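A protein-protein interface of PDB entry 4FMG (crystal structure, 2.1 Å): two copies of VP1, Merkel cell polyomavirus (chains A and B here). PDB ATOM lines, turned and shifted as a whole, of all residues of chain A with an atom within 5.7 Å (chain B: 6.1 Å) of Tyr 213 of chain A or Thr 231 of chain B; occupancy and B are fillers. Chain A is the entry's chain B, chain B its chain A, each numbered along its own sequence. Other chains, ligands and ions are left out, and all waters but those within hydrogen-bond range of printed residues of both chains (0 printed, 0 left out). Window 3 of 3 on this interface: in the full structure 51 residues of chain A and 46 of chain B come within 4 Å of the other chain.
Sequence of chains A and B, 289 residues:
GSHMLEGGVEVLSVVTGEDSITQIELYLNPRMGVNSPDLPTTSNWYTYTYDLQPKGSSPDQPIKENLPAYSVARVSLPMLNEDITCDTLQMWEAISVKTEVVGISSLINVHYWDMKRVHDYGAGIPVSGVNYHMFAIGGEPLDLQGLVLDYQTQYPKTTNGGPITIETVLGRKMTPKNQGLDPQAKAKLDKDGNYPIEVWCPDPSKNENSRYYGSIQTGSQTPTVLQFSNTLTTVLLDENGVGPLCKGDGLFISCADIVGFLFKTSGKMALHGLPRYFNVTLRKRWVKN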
ATOM      1  N   HIS A 133      -3.734  20.388  34.745  1.00  0.00           N
ATOM      2  CA  HIS A 133      -3.014  19.365  33.987  1.00  0.00           C
ATOM      3  C   HIS A 133      -3.865  18.791  32.890  1.00  0.00           C
ATOM      4  O   HIS A 133      -4.946  18.267  33.138  1.00  0.00           O
ATOM      5  CB  HIS A 133      -2.519  18.240  34.899  1.00  0.00           C
ATOM      6  CG  HIS A 133      -1.559  18.711  35.932  1.00  0.00           C
ATOM      7  ND1 HIS A 133      -0.216  18.869  35.677  1.00  0.00           N
ATOM      8  CD2 HIS A 133      -1.756  19.132  37.205  1.00  0.00           C
ATOM      9  CE1 HIS A 133       0.384  19.329  36.760  1.00  0.00           C
ATOM     10  NE2 HIS A 133      -0.529  19.502  37.700  1.00  0.00           N
ATOM     11  N   MET A 134      -3.374  18.893  31.668  1.00  0.00           N
ATOM     12  CA  MET A 134      -4.051  18.271  30.547  1.00  0.00           C
ATOM     13  C   MET A 134      -3.036  17.882  29.487  1.00  0.00           C
ATOM     14  O   MET A 134      -1.990  18.527  29.350  1.00  0.00           O
ATOM     15  CB  MET A 134      -5.128  19.212  29.973  1.00  0.00           C
ATOM     16  CG  MET A 134      -4.616  20.359  29.113  1.00  0.00           C
ATOM     17  SD  MET A 134      -4.515  20.014  27.326  1.00  0.00           S
ATOM     18  CE  MET A 134      -6.240  19.751  26.936  1.00  0.00           C
ATOM     19  N   PHE A 135      -3.341  16.816  28.757  1.00  0.00           N
ATOM     20  CA  PHE A 135      -2.670  16.549  27.500  1.00  0.00           C
ATOM     21  C   PHE A 135      -3.704  16.104  26.465  1.00  0.00           C
ATOM     22  O   PHE A 135      -4.829  15.709  26.820  1.00  0.00           O
ATOM     23  CB  PHE A 135      -1.540  15.528  27.662  1.00  0.00           C
ATOM     24  CG  PHE A 135      -2.014  14.111  27.894  1.00  0.00           C
ATOM     25  CD1 PHE A 135      -2.346  13.673  29.176  1.00  0.00           C
ATOM     26  CD2 PHE A 135      -2.109  13.210  26.831  1.00  0.00           C
ATOM     27  CE1 PHE A 135      -2.775  12.362  29.395  1.00  0.00           C
ATOM     28  CE2 PHE A 135      -2.550  11.901  27.040  1.00  0.00           C
ATOM     29  CZ  PHE A 135      -2.872  11.474  28.319  1.00  0.00           C
ATOM     30  N   ALA A 136      -3.319  16.194  25.192  1.00  0.00           N
ATOM     31  CA  ALA A 136      -4.169  15.790  24.073  1.00  0.00           C
ATOM     32  C   ALA A 136      -3.318  15.234  22.938  1.00  0.00           C
ATOM     33  O   ALA A 136      -2.215  15.731  22.681  1.00  0.00           O
ATOM     34  CB  ALA A 136      -5.014  16.980  23.569  1.00  0.00           C
ATOM     35  N   ARG A 211      -7.909  12.926  21.247  1.00  0.00           N
ATOM     36  CA  ARG A 211      -8.175  12.402  22.587  1.00  0.00           C
ATOM     37  C   ARG A 211      -7.556  13.371  23.584  1.00  0.00           C
ATOM     38  O   ARG A 211      -6.353  13.629  23.523  1.00  0.00           O
ATOM     39  CB  ARG A 211      -7.555  11.013  22.770  1.00  0.00           C
ATOM     40  CG  ARG A 211      -7.875   9.997  21.662  1.00  0.00           C
ATOM     41  CD  ARG A 211      -9.354   9.627  21.614  1.00  0.00           C
ATOM     42  NE  ARG A 211      -9.639   8.713  20.506  1.00  0.00           N
ATOM     43  CZ  ARG A 211     -10.106   9.068  19.307  1.00  0.00           C
ATOM     44  NH1 ARG A 211     -10.378  10.338  19.021  1.00  0.00           N
ATOM     45  NH2 ARG A 211     -10.302   8.136  18.383  1.00  0.00           N
ATOM     46  N   TYR A 212      -8.364  13.931  24.487  1.00  0.00           N
ATOM     47  CA  TYR A 212      -7.821  14.822  25.526  1.00  0.00           C
ATOM     48  C   TYR A 212      -8.254  14.400  26.938  1.00  0.00           C
ATOM     49  O   TYR A 212      -9.325  13.810  27.122  1.00  0.00           O
ATOM     50  CB  TYR A 212      -8.130  16.311  25.244  1.00  0.00           C
ATOM     51  CG  TYR A 212      -9.602  16.674  25.323  1.00  0.00           C
ATOM     52  CD1 TYR A 212     -10.233  16.884  26.557  1.00  0.00           C
ATOM     53  CD2 TYR A 212     -10.363  16.815  24.166  1.00  0.00           C
ATOM     54  CE1 TYR A 212     -11.597  17.209  26.628  1.00  0.00           C
ATOM     55  CE2 TYR A 212     -11.726  17.138  24.226  1.00  0.00           C
ATOM     56  CZ  TYR A 212     -12.331  17.339  25.455  1.00  0.00           C
ATOM     57  OH  TYR A 212     -13.673  17.656  25.497  1.00  0.00           O
ATOM     58  N   TYR A 213      -7.395  14.696  27.917  1.00  0.00           N
ATOM     59  CA  TYR A 213      -7.592  14.299  29.310  1.00  0.00           C
ATOM     60  C   TYR A 213      -7.043  15.410  30.174  1.00  0.00           C
ATOM     61  O   TYR A 213      -5.883  15.806  30.011  1.00  0.00           O
ATOM     62  CB  TYR A 213      -6.810  13.011  29.633  1.00  0.00           C
ATOM     63  CG  TYR A 213      -6.884  11.925  28.578  1.00  0.00           C
ATOM     64  CD1 TYR A 213      -7.728  10.830  28.733  1.00  0.00           C
ATOM     65  CD2 TYR A 213      -6.097  11.989  27.426  1.00  0.00           C
ATOM     66  CE1 TYR A 213      -7.786   9.819  27.762  1.00  0.00           C
ATOM     67  CE2 TYR A 213      -6.155  11.005  26.453  1.00  0.00           C
ATOM     68  CZ  TYR A 213      -6.997   9.920  26.622  1.00  0.00           C
ATOM     69  OH  TYR A 213      -7.038   8.934  25.641  1.00  0.00           O
ATOM     70  N   GLY A 214      -7.860  15.916  31.093  1.00  0.00           N
ATOM     71  CA  GLY A 214      -7.399  16.984  31.967  1.00  0.00           C
ATOM     72  C   GLY A 214      -8.036  17.086  33.341  1.00  0.00           C
ATOM     73  O   GLY A 214      -9.039  16.424  33.639  1.00  0.00           O
ATOM     74  N   SER A 215      -7.441  17.936  34.173  1.00  0.00           N
ATOM     75  CA  SER A 215      -7.958  18.212  35.509  1.00  0.00           C
ATOM     76  C   SER A 215      -7.519  19.589  35.986  1.00  0.00           C
ATOM     77  O   SER A 215      -6.507  20.136  35.511  1.00  0.00           O
ATOM     78  CB  SER A 215      -7.504  17.131  36.499  1.00  0.00           C
ATOM     79  OG  SER A 215      -6.095  17.156  36.659  1.00  0.00           O
ATOM     80  N   THR A 234      -1.657   5.171  28.097  1.00  0.00           N
ATOM     81  CA  THR A 234      -3.021   5.536  27.730  1.00  0.00           C
ATOM     82  C   THR A 234      -3.348   4.994  26.338  1.00  0.00           C
ATOM     83  O   THR A 234      -2.637   5.279  25.379  1.00  0.00           O
ATOM     84  CB  THR A 234      -3.244   7.058  27.793  1.00  0.00           C
ATOM     85  OG1 THR A 234      -2.959   7.527  29.117  1.00  0.00           O
ATOM     86  CG2 THR A 234      -4.685   7.411  27.441  1.00  0.00           C
ATOM     87  N   VAL A 235      -4.414   4.200  26.251  1.00  0.00           N
ATOM     88  CA  VAL A 235      -4.945   3.714  24.978  1.00  0.00           C
ATOM     89  C   VAL A 235      -5.785   4.825  24.319  1.00  0.00           C
ATOM     90  O   VAL A 235      -6.635   5.448  24.963  1.00  0.00           O
ATOM     91  CB  VAL A 235      -5.760   2.410  25.168  1.00  0.00           C
ATOM     92  CG1 VAL A 235      -6.482   1.994  23.883  1.00  0.00           C
ATOM     93  CG2 VAL A 235      -4.851   1.272  25.668  1.00  0.00           C
ATOM     94  N   LEU A 236      -5.522   5.066  23.032  1.00  0.00           N
ATOM     95  CA  LEU A 236      -6.096   6.202  22.306  1.00  0.00           C
ATOM     96  C   LEU A 236      -7.264   5.833  21.381  1.00  0.00           C
ATOM     97  O   LEU A 236      -7.833   6.700  20.722  1.00  0.00           O
ATOM     98  CB  LEU A 236      -5.000   6.913  21.506  1.00  0.00           C
ATOM     99  CG  LEU A 236      -3.868   7.565  22.303  1.00  0.00           C
ATOM    100  CD1 LEU A 236      -2.736   7.969  21.377  1.00  0.00           C
ATOM    101  CD2 LEU A 236      -4.366   8.771  23.115  1.00  0.00           C
ATOM    102  N   LYS B  98     -22.116  11.246  26.562  1.00  0.00           N
ATOM    103  CA  LYS B  98     -20.857  11.891  26.902  1.00  0.00           C
ATOM    104  C   LYS B  98     -21.206  13.267  27.408  1.00  0.00           C
ATOM    105  O   LYS B  98     -21.852  14.051  26.704  1.00  0.00           O
ATOM    106  CB  LYS B  98     -19.926  12.012  25.698  1.00  0.00           C
ATOM    107  CG  LYS B  98     -19.323  10.705  25.240  1.00  0.00           C
ATOM    108  CD  LYS B  98     -18.357  10.947  24.088  1.00  0.00           C
ATOM    109  CE  LYS B  98     -17.353   9.825  23.991  1.00  0.00           C
ATOM    110  NZ  LYS B  98     -16.324  10.125  22.971  1.00  0.00           N
ATOM    111  N   PHE B 228     -11.926  16.577  33.024  1.00  0.00           N
ATOM    112  CA  PHE B 228     -12.519  16.712  31.696  1.00  0.00           C
ATOM    113  C   PHE B 228     -11.788  15.818  30.695  1.00  0.00           C
ATOM    114  O   PHE B 228     -10.561  15.816  30.635  1.00  0.00           O
ATOM    115  CB  PHE B 228     -12.560  18.186  31.219  1.00  0.00           C
ATOM    116  CG  PHE B 228     -11.228  18.885  31.275  1.00  0.00           C
ATOM    117  CD1 PHE B 228     -10.756  19.418  32.473  1.00  0.00           C
ATOM    118  CD2 PHE B 228     -10.450  19.016  30.132  1.00  0.00           C
ATOM    119  CE1 PHE B 228      -9.522  20.056  32.535  1.00  0.00           C
ATOM    120  CE2 PHE B 228      -9.212  19.653  30.179  1.00  0.00           C
ATOM    121  CZ  PHE B 228      -8.746  20.175  31.379  1.00  0.00           C
ATOM    122  N   SER B 229     -12.561  15.044  29.939  1.00  0.00           N
ATOM    123  CA  SER B 229     -12.031  14.166  28.899  1.00  0.00           C
ATOM    124  C   SER B 229     -13.137  13.822  27.902  1.00  0.00           C
ATOM    125  O   SER B 229     -14.267  13.556  28.304  1.00  0.00           O
ATOM    126  CB  SER B 229     -11.483  12.873  29.513  1.00  0.00           C
ATOM    127  OG  SER B 229     -10.969  12.002  28.515  1.00  0.00           O
ATOM    128  N   ASN B 230     -12.807  13.797  26.611  1.00  0.00           N
ATOM    129  CA  ASN B 230     -13.769  13.329  25.616  1.00  0.00           C
ATOM    130  C   ASN B 230     -13.774  11.806  25.418  1.00  0.00           C
ATOM    131  O   ASN B 230     -14.377  11.307  24.462  1.00  0.00           O
ATOM    132  CB  ASN B 230     -13.604  14.067  24.280  1.00  0.00           C
ATOM    133  CG  ASN B 230     -12.281  13.761  23.586  1.00  0.00           C
ATOM    134  OD1 ASN B 230     -11.306  13.327  24.218  1.00  0.00           O
ATOM    135  ND2 ASN B 230     -12.239  13.993  22.274  1.00  0.00           N
ATOM    136  N   THR B 231     -13.111  11.074  26.320  1.00  0.00           N
ATOM    137  CA  THR B 231     -13.024   9.608  26.220  1.00  0.00           C
ATOM    138  C   THR B 231     -13.956   8.892  27.197  1.00  0.00           C
ATOM    139  O   THR B 231     -13.953   7.664  27.265  1.00  0.00           O
ATOM    140  CB  THR B 231     -11.587   9.092  26.455  1.00  0.00           C
ATOM    141  OG1 THR B 231     -11.206   9.340  27.818  1.00  0.00           O
ATOM    142  CG2 THR B 231     -10.603   9.776  25.520  1.00  0.00           C
ATOM    143  N   LEU B 232     -14.746   9.655  27.952  1.00  0.00           N
ATOM    144  CA  LEU B 232     -15.578   9.078  29.013  1.00  0.00           C
ATOM    145  C   LEU B 232     -17.059   9.006  28.670  1.00  0.00           C
ATOM    146  O   LEU B 232     -17.687  10.028  28.418  1.00  0.00           O
ATOM    147  CB  LEU B 232     -15.381   9.845  30.327  1.00  0.00           C
ATOM    148  CG  LEU B 232     -14.004   9.723  30.990  1.00  0.00           C
ATOM    149  CD1 LEU B 232     -13.939  10.598  32.231  1.00  0.00           C
ATOM    150  CD2 LEU B 232     -13.645   8.261  31.325  1.00  0.00           C
ATOM    151  N   THR B 233     -17.607   7.793  28.701  1.00  0.00           N
ATOM    152  CA  THR B 233     -19.010   7.537  28.370  1.00  0.00           C
ATOM    153  C   THR B 233     -19.797   6.977  29.567  1.00  0.00           C
ATOM    154  O   THR B 233     -19.315   6.092  30.278  1.00  0.00           O
ATOM    155  CB  THR B 233     -19.119   6.535  27.176  1.00  0.00           C
ATOM    156  OG1 THR B 233     -18.344   7.012  26.067  1.00  0.00           O
ATOM    157  CG2 THR B 233     -20.569   6.349  26.729  1.00  0.00           C
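Thr 231 of chain B touches one residue of chain A.
Of the printed residues of chain A, Ser 229 of chain B touches Tyr 212 and Tyr 213.
Of the printed residues of chain A, Phe 228 of chain B touches Met 134 (3.999 Å), Tyr 213 (3.6 Å), Gly 214 (2.7 Å) and Ser 215 (3.4 Å).
Printed residues of chain B within 4 Å of Gly 214 of chain A: Phe 228 (2.7 Å).
Val 235 of chain A touches none of the printed residues of chain B.
Ala 136 of chain A touches none of the printed residues of chain B.
The nearest residue of chain B that does not touch Tyr 213 of chain A is Asn 230 of chain B (5.6 Å).
The nearest residue of chain A that does not touch Thr 231 of chain B is Arg 211 of chain A (4.1 Å).
The nearest printed residue of chain B that does not touch Ser 215 of chain A is Ser 229 of chain B (7.2 Å).
No position is printed for both chains.
Hydrophobic or aromatic side chains of chain A that line the printed part of chain B: Met 134, Tyr 212 and Tyr 213.
Of the 7 printed residues of chain B, 4 touch a printed residue of chain A.
Hydrophobic or aromatic side chains of chain B that line the printed part of chain A: Phe 228.
Among the printed residues, pairs that only touch across the chains: Ser 215 of chain A with Phe 228 of chain B (3.4 Å), Tyr 213 of chain A with Ser 229 of chain B (3.5 Å), Tyr 213 of chain A with Thr 231 of chain B (3.5 Å), Tyr 213 of chain A with Phe 228 of chain B (3.6 Å), Arg 211 of chain A with Asn 230 of chain B (3.6 Å) and Met 134 of chain A with Phe 228 of chain B (3.999 Å).
The backbone carbonyl oxygen (O) of Asn 230 of chain B lies within hydrogen-bond range of the side-chain amino group (NZ) of Lys 98 of chain B (2.7 Å).
The side-chain hydroxyl (OG) of Ser 229 of chain B is in hydrogen-bond range of the side-chain hydroxyl (OG1) of Thr 231 of chain B (2.8 Å).
N of Ser 215 of chain A sits at hydrogen-bond distance from O of His 133 of chain A.
The backbone carbonyl oxygen (O) of Phe 135 of chain A is in hydrogen-bond range of the backbone NH (N) of Tyr 213 of chain A (3.0 Å).
The guanidinium group (NE) of Arg 211 of chain A is in hydrogen-bond range of the backbone carbonyl oxygen (O) of Leu 236 of chain A (2.7 Å).
The side-chain amide oxygen of Asn 230 of chain B lies within hydrogen-bond range of the backbone NH of Tyr 212 of chain A, at 3.0 Å.
O of Tyr 212 of chain A sits at hydrogen-bond distance from OG of Ser 229 of chain B.
The backbone carbonyl oxygen (O) of Phe 228 of chain B lies within hydrogen-bond range of the backbone NH (N) of Gly 214 of chain A (2.7 Å).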
